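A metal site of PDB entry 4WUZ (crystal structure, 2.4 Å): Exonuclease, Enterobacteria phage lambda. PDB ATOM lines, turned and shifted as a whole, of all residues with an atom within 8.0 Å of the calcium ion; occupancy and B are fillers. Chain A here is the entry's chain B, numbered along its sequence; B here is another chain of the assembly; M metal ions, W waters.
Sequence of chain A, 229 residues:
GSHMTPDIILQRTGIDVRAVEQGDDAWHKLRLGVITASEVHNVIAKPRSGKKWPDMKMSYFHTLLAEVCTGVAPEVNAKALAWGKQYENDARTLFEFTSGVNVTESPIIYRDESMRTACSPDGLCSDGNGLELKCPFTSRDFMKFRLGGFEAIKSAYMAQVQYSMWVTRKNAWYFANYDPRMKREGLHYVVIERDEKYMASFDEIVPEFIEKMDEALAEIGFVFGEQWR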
ATOM      1  N   SER A  38      16.987  24.633  -1.362  1.00  0.00           N
ATOM      2  CA  SER A  38      18.433  24.504  -1.707  1.00  0.00           C
ATOM      3  C   SER A  38      19.360  25.106  -0.658  1.00  0.00           C
ATOM      4  O   SER A  38      20.575  24.927  -0.775  1.00  0.00           O
ATOM      5  CB  SER A  38      18.755  25.155  -3.062  1.00  0.00           C
ATOM      6  OG  SER A  38      18.366  26.539  -3.052  1.00  0.00           O
ATOM      7  N   GLY A  84      23.647  24.154 -15.610  1.00  0.00           N
ATOM      8  CA  GLY A  84      22.472  23.655 -14.875  1.00  0.00           C
ATOM      9  C   GLY A  84      21.139  24.251 -15.318  1.00  0.00           C
ATOM     10  O   GLY A  84      20.134  23.541 -15.392  1.00  0.00           O
ATOM     11  N   GLU A  88      18.259  21.709 -17.710  1.00  0.00           N
ATOM     12  CA  GLU A  88      17.106  21.329 -16.915  1.00  0.00           C
ATOM     13  C   GLU A  88      15.839  20.866 -17.692  1.00  0.00           C
ATOM     14  O   GLU A  88      15.271  19.837 -17.346  1.00  0.00           O
ATOM     15  CB  GLU A  88      16.757  22.477 -15.989  1.00  0.00           C
ATOM     16  CG  GLU A  88      15.782  22.063 -14.949  1.00  0.00           C
ATOM     17  CD  GLU A  88      14.935  23.207 -14.547  1.00  0.00           C
ATOM     18  OE1 GLU A  88      15.456  24.079 -13.834  1.00  0.00           O
ATOM     19  OE2 GLU A  88      13.772  23.237 -14.984  1.00  0.00           O
ATOM     20  N   ARG A  92      14.309  17.087 -17.784  1.00  0.00           N
ATOM     21  CA  ARG A  92      12.929  16.832 -17.396  1.00  0.00           C
ATOM     22  C   ARG A  92      12.268  15.985 -18.482  1.00  0.00           C
ATOM     23  O   ARG A  92      11.647  14.972 -18.175  1.00  0.00           O
ATOM     24  CB  ARG A  92      12.157  18.154 -17.143  1.00  0.00           C
ATOM     25  CG  ARG A  92      10.612  18.014 -17.039  1.00  0.00           C
ATOM     26  CD  ARG A  92       9.948  19.053 -16.119  1.00  0.00           C
ATOM     27  NE  ARG A  92      10.366  20.411 -16.440  1.00  0.00           N
ATOM     28  CZ  ARG A  92      11.072  21.224 -15.647  1.00  0.00           C
ATOM     29  NH1 ARG A  92      11.437  20.851 -14.445  1.00  0.00           N
ATOM     30  NH2 ARG A  92      11.407  22.442 -16.085  1.00  0.00           N
ATOM     31  N   SER A 120      11.086  25.236  -4.477  1.00  0.00           N
ATOM     32  CA  SER A 120      10.646  25.280  -5.889  1.00  0.00           C
ATOM     33  C   SER A 120      10.975  23.959  -6.570  1.00  0.00           C
ATOM     34  O   SER A 120      12.088  23.652  -6.885  1.00  0.00           O
ATOM     35  CB  SER A 120      11.107  26.522  -6.617  1.00  0.00           C
ATOM     36  OG  SER A 120      12.083  27.183  -5.824  1.00  0.00           O
ATOM     37  N   PRO A 121       9.988  23.116  -6.662  1.00  0.00           N
ATOM     38  CA  PRO A 121      10.288  21.827  -7.215  1.00  0.00           C
ATOM     39  C   PRO A 121      10.651  21.904  -8.716  1.00  0.00           C
ATOM     40  O   PRO A 121      10.099  22.747  -9.475  1.00  0.00           O
ATOM     41  CB  PRO A 121       8.960  21.052  -7.038  1.00  0.00           C
ATOM     42  CG  PRO A 121       8.210  21.786  -5.964  1.00  0.00           C
ATOM     43  CD  PRO A 121       8.707  23.176  -5.914  1.00  0.00           C
ATOM     44  N   ASP A 122      11.558  21.039  -9.142  1.00  0.00           N
ATOM     45  CA  ASP A 122      11.743  20.818 -10.560  1.00  0.00           C
ATOM     46  C   ASP A 122      10.531  20.130 -11.203  1.00  0.00           C
ATOM     47  O   ASP A 122      10.512  19.966 -12.410  1.00  0.00           O
ATOM     48  CB  ASP A 122      13.031  20.055 -10.835  1.00  0.00           C
ATOM     49  CG  ASP A 122      14.258  20.871 -10.460  1.00  0.00           C
ATOM     50  OD1 ASP A 122      14.079  22.069 -10.305  1.00  0.00           O
ATOM     51  OD2 ASP A 122      15.373  20.338 -10.286  1.00  0.00           O
ATOM     52  N   GLY A 123       9.531  19.718 -10.400  1.00  0.00           N
ATOM     53  CA  GLY A 123       8.242  19.286 -10.935  1.00  0.00           C
ATOM     54  C   GLY A 123       7.408  18.442  -9.972  1.00  0.00           C
ATOM     55  O   GLY A 123       7.866  17.992  -8.889  1.00  0.00           O
ATOM     56  N   LEU A 131       9.859  16.154  -7.927  1.00  0.00           N
ATOM     57  CA  LEU A 131      11.024  15.861  -8.719  1.00  0.00           C
ATOM     58  C   LEU A 131      12.087  16.888  -8.496  1.00  0.00           C
ATOM     59  O   LEU A 131      11.823  18.094  -8.609  1.00  0.00           O
ATOM     60  CB  LEU A 131      10.647  15.790 -10.206  1.00  0.00           C
ATOM     61  CG  LEU A 131      11.747  15.826 -11.292  1.00  0.00           C
ATOM     62  CD1 LEU A 131      12.421  14.552 -11.267  1.00  0.00           C
ATOM     63  CD2 LEU A 131      11.199  16.073 -12.721  1.00  0.00           C
ATOM     64  N   GLU A 132      13.276  16.407  -8.170  1.00  0.00           N
ATOM     65  CA  GLU A 132      14.494  17.202  -8.187  1.00  0.00           C
ATOM     66  C   GLU A 132      15.429  16.775  -9.351  1.00  0.00           C
ATOM     67  O   GLU A 132      15.845  15.602  -9.426  1.00  0.00           O
ATOM     68  CB  GLU A 132      15.184  17.140  -6.825  1.00  0.00           C
ATOM     69  CG  GLU A 132      16.461  18.040  -6.658  1.00  0.00           C
ATOM     70  CD  GLU A 132      16.251  19.493  -7.086  1.00  0.00           C
ATOM     71  OE1 GLU A 132      15.143  20.036  -6.875  1.00  0.00           O
ATOM     72  OE2 GLU A 132      17.220  20.106  -7.612  1.00  0.00           O
ATOM     73  N   LEU A 133      15.655  17.710 -10.289  1.00  0.00           N
ATOM     74  CA  LEU A 133      16.620  17.632 -11.421  1.00  0.00           C
ATOM     75  C   LEU A 133      17.977  18.321 -11.177  1.00  0.00           C
ATOM     76  O   LEU A 133      18.040  19.524 -10.803  1.00  0.00           O
ATOM     77  CB  LEU A 133      16.034  18.390 -12.612  1.00  0.00           C
ATOM     78  CG  LEU A 133      15.329  17.702 -13.788  1.00  0.00           C
ATOM     79  CD1 LEU A 133      14.961  16.238 -13.570  1.00  0.00           C
ATOM     80  CD2 LEU A 133      14.164  18.588 -14.212  1.00  0.00           C
ATOM     81  N   LYS A 134      19.061  17.579 -11.398  1.00  0.00           N
ATOM     82  CA  LYS A 134      20.422  18.095 -11.376  1.00  0.00           C
ATOM     83  C   LYS A 134      20.969  17.792 -12.751  1.00  0.00           C
ATOM     84  O   LYS A 134      20.709  16.749 -13.322  1.00  0.00           O
ATOM     85  CB  LYS A 134      21.304  17.383 -10.337  1.00  0.00           C
ATOM     86  CG  LYS A 134      20.783  17.299  -8.876  1.00  0.00           C
ATOM     87  CD  LYS A 134      20.929  18.648  -8.185  1.00  0.00           C
ATOM     88  CE  LYS A 134      20.085  18.775  -6.948  1.00  0.00           C
ATOM     89  NZ  LYS A 134      19.950  20.195  -6.462  1.00  0.00           N
ATOM     90  N   CYS A 135      21.723  18.746 -13.279  1.00  0.00           N
ATOM     91  CA  CYS A 135      22.479  18.586 -14.505  1.00  0.00           C
ATOM     92  C   CYS A 135      23.871  18.989 -14.122  1.00  0.00           C
ATOM     93  O   CYS A 135      24.260  20.141 -14.306  1.00  0.00           O
ATOM     94  CB  CYS A 135      21.935  19.528 -15.581  1.00  0.00           C
ATOM     95  SG  CYS A 135      20.208  19.182 -16.002  1.00  0.00           S
ATOM     96  N   GLN A 160      17.934  19.195   0.857  1.00  0.00           N
ATOM     97  CA  GLN A 160      17.051  19.869  -0.087  1.00  0.00           C
ATOM     98  C   GLN A 160      15.777  19.057  -0.415  1.00  0.00           C
ATOM     99  O   GLN A 160      14.648  19.631  -0.437  1.00  0.00           O
ATOM    100  CB  GLN A 160      17.807  20.268  -1.367  1.00  0.00           C
ATOM    101  CG  GLN A 160      16.885  20.685  -2.523  1.00  0.00           C
ATOM    102  CD  GLN A 160      17.595  21.180  -3.765  1.00  0.00           C
ATOM    103  OE1 GLN A 160      18.756  20.828  -4.045  1.00  0.00           O
ATOM    104  NE2 GLN A 160      16.887  21.958  -4.562  1.00  0.00           N
ATOM    105  N   PHE A 175      14.756  11.936  -7.606  1.00  0.00           N
ATOM    106  CA  PHE A 175      16.096  12.547  -7.701  1.00  0.00           C
ATOM    107  C   PHE A 175      16.794  12.003  -8.938  1.00  0.00           C
ATOM    108  O   PHE A 175      17.286  10.875  -8.911  1.00  0.00           O
ATOM    109  CB  PHE A 175      16.962  12.233  -6.466  1.00  0.00           C
ATOM    110  CG  PHE A 175      18.253  13.046  -6.407  1.00  0.00           C
ATOM    111  CD1 PHE A 175      19.477  12.448  -6.741  1.00  0.00           C
ATOM    112  CD2 PHE A 175      18.233  14.386  -6.011  1.00  0.00           C
ATOM    113  CE1 PHE A 175      20.664  13.187  -6.712  1.00  0.00           C
ATOM    114  CE2 PHE A 175      19.429  15.162  -5.964  1.00  0.00           C
ATOM    115  CZ  PHE A 175      20.643  14.549  -6.327  1.00  0.00           C
ATOM    116  N   ALA A 176      16.827  12.835  -9.985  1.00  0.00           N
ATOM    117  CA  ALA A 176      17.354  12.548 -11.301  1.00  0.00           C
ATOM    118  C   ALA A 176      18.583  13.425 -11.588  1.00  0.00           C
ATOM    119  O   ALA A 176      18.621  14.619 -11.249  1.00  0.00           O
ATOM    120  CB  ALA A 176      16.304  12.825 -12.357  1.00  0.00           C
ATOM    121  OP3  DA B   1      15.838  27.045  -2.892  1.00  0.00           O
ATOM    122  P    DA B   1      14.768  26.465  -3.738  1.00  0.00           P
ATOM    123  OP1  DA B   1      14.148  25.273  -3.135  1.00  0.00           O
ATOM    124  OP2  DA B   1      13.767  27.507  -4.018  1.00  0.00           O
ATOM    125  O5'  DA B   1      15.609  26.130  -5.075  1.00  0.00           O
ATOM    126  C5'  DA B   1      16.097  27.224  -5.889  1.00  0.00           C
ATOM    127  C4'  DA B   1      17.026  26.780  -7.015  1.00  0.00           C
ATOM    128  O4'  DA B   1      17.173  27.757  -8.100  1.00  0.00           O
ATOM    129  C3'  DA B   1      18.411  26.400  -6.513  1.00  0.00           C
ATOM    130  O3'  DA B   1      18.549  25.054  -7.017  1.00  0.00           O
ATOM    131  C2'  DA B   1      19.299  27.520  -7.048  1.00  0.00           C
ATOM    132  C1'  DA B   1      18.543  28.069  -8.271  1.00  0.00           C
ATOM    133  N9   DA B   1      18.755  29.506  -8.541  1.00  0.00           N
ATOM    134  C8   DA B   1      19.095  30.477  -7.633  1.00  0.00           C
ATOM    135  N7   DA B   1      19.232  31.684  -8.151  1.00  0.00           N
ATOM    136  C5   DA B   1      18.976  31.508  -9.500  1.00  0.00           C
ATOM    137  C6   DA B   1      18.966  32.385 -10.618  1.00  0.00           C
ATOM    138  N6   DA B   1      19.235  33.697 -10.563  1.00  0.00           N
ATOM    139  N1   DA B   1      18.666  31.881 -11.836  1.00  0.00           N
ATOM    140  C2   DA B   1      18.409  30.565 -11.953  1.00  0.00           C
ATOM    141  N3   DA B   1      18.390  29.638 -10.984  1.00  0.00           N
ATOM    142  C4   DA B   1      18.686  30.167  -9.763  1.00  0.00           C
ATOM    143  P    DG B   2      19.837  24.084  -7.184  1.00  0.00           P
ATOM    144  OP1  DG B   2      19.259  22.796  -7.695  1.00  0.00           O
ATOM    145  OP2  DG B   2      20.776  24.056  -6.006  1.00  0.00           O
ATOM    146  O5'  DG B   2      20.546  24.901  -8.391  1.00  0.00           O
ATOM    147  C5'  DG B   2      19.697  25.482  -9.473  1.00  0.00           C
ATOM    148  C4'  DG B   2      20.468  25.498 -10.768  1.00  0.00           C
ATOM    149  O4'  DG B   2      20.835  26.834 -11.217  1.00  0.00           O
ATOM    150  C3'  DG B   2      21.743  24.731 -10.476  1.00  0.00           C
ATOM    151  O3'  DG B   2      21.717  23.631 -11.368  1.00  0.00           O
ATOM    152  C2'  DG B   2      22.871  25.739 -10.670  1.00  0.00           C
ATOM    153  C1'  DG B   2      22.167  27.097 -10.783  1.00  0.00           C
ATOM    154  N9   DG B   2      22.240  27.961  -9.566  1.00  0.00           N
ATOM    155  C8   DG B   2      22.324  27.579  -8.229  1.00  0.00           C
ATOM    156  N7   DG B   2      22.386  28.582  -7.386  1.00  0.00           N
ATOM    157  C5   DG B   2      22.359  29.722  -8.195  1.00  0.00           C
ATOM    158  C6   DG B   2      22.406  31.106  -7.870  1.00  0.00           C
ATOM    159  O6   DG B   2      22.476  31.613  -6.743  1.00  0.00           O
ATOM    160  N1   DG B   2      22.348  31.931  -9.006  1.00  0.00           N
ATOM    161  C2   DG B   2      22.265  31.486 -10.317  1.00  0.00           C
ATOM    162  N2   DG B   2      22.219  32.418 -11.283  1.00  0.00           N
ATOM    163  N3   DG B   2      22.220  30.190 -10.641  1.00  0.00           N
ATOM    164  C4   DG B   2      22.267  29.355  -9.544  1.00  0.00           C
ATOM    165  P    DC B   3      22.160  22.180 -10.894  1.00  0.00           P
ATOM    166  OP1  DC B   3      21.915  21.182 -11.986  1.00  0.00           O
ATOM    167  OP2  DC B   3      21.496  21.944  -9.578  1.00  0.00           O
ATOM    168  O5'  DC B   3      23.739  22.455 -10.700  1.00  0.00           O
ATOM    169  C5'  DC B   3      24.596  22.605 -11.801  1.00  0.00           C
ATOM    170  C4'  DC B   3      25.989  22.566 -11.242  1.00  0.00           C
ATOM    171  O4'  DC B   3      26.238  23.765 -10.493  1.00  0.00           O
ATOM    172  C3'  DC B   3      26.291  21.420 -10.308  1.00  0.00           C
ATOM    173  O3'  DC B   3      27.517  20.924 -10.783  1.00  0.00           O
ATOM    174  C2'  DC B   3      26.370  22.074  -8.928  1.00  0.00           C
ATOM    175  C1'  DC B   3      26.870  23.463  -9.284  1.00  0.00           C
ATOM    176  N1   DC B   3      26.508  24.597  -8.374  1.00  0.00           N
ATOM    177  C2   DC B   3      27.447  25.656  -8.271  1.00  0.00           C
ATOM    178  O2   DC B   3      28.531  25.591  -8.900  1.00  0.00           O
ATOM    179  N3   DC B   3      27.142  26.733  -7.485  1.00  0.00           N
ATOM    180  C4   DC B   3      25.958  26.779  -6.835  1.00  0.00           C
ATOM    181  N4   DC B   3      25.741  27.858  -6.077  1.00  0.00           N
ATOM    182  C5   DC B   3      24.967  25.706  -6.934  1.00  0.00           C
ATOM    183  C6   DC B   3      25.280  24.656  -7.731  1.00  0.00           C
HETATM  184 CA    CA M   1      17.061  21.594  -9.536  1.00  0.00          CA
HETATM  185  O   HOH W   1      16.597  23.551  -8.922  1.00  0.00           O
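The side-chain carboxylate (OE1) of Glu 132 is in hydrogen-bond range of the side-chain amide nitrogen (NE2) of Gln 160.
The backbone NH (N) of Ala 176 lies within hydrogen-bond range of the backbone carbonyl oxygen (O) of Glu 132.
The side-chain carboxylate of Glu 132 lies close to the side-chain amino group of Lys 134.
The backbone carbonyl oxygen of Leu 131 sits at hydrogen-bond distance from the backbone NH of Asp 122, 3.0 Å away.
OP1 of DG 2 of chain B is in salt-bridge range of the side-chain amino group (NZ) of Lys 134 (3.0 Å).
O of Asp 122 lies within hydrogen-bond range of NH1 of Arg 92, at 2.4 Å.
The calcium ion is bound by water W1 (2.1 Å), OD2 of Asp 122 (2.2 Å), OE2 of Glu 132 (2.4 Å) and O of Leu 133 (2.6 Å).
Slightly farther from the calcium ion lies OP1 of DG 2 of chain B (3.1 Å).
Slightly farther from the calcium ion lies OD1 of Asp 122 (3.1 Å).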
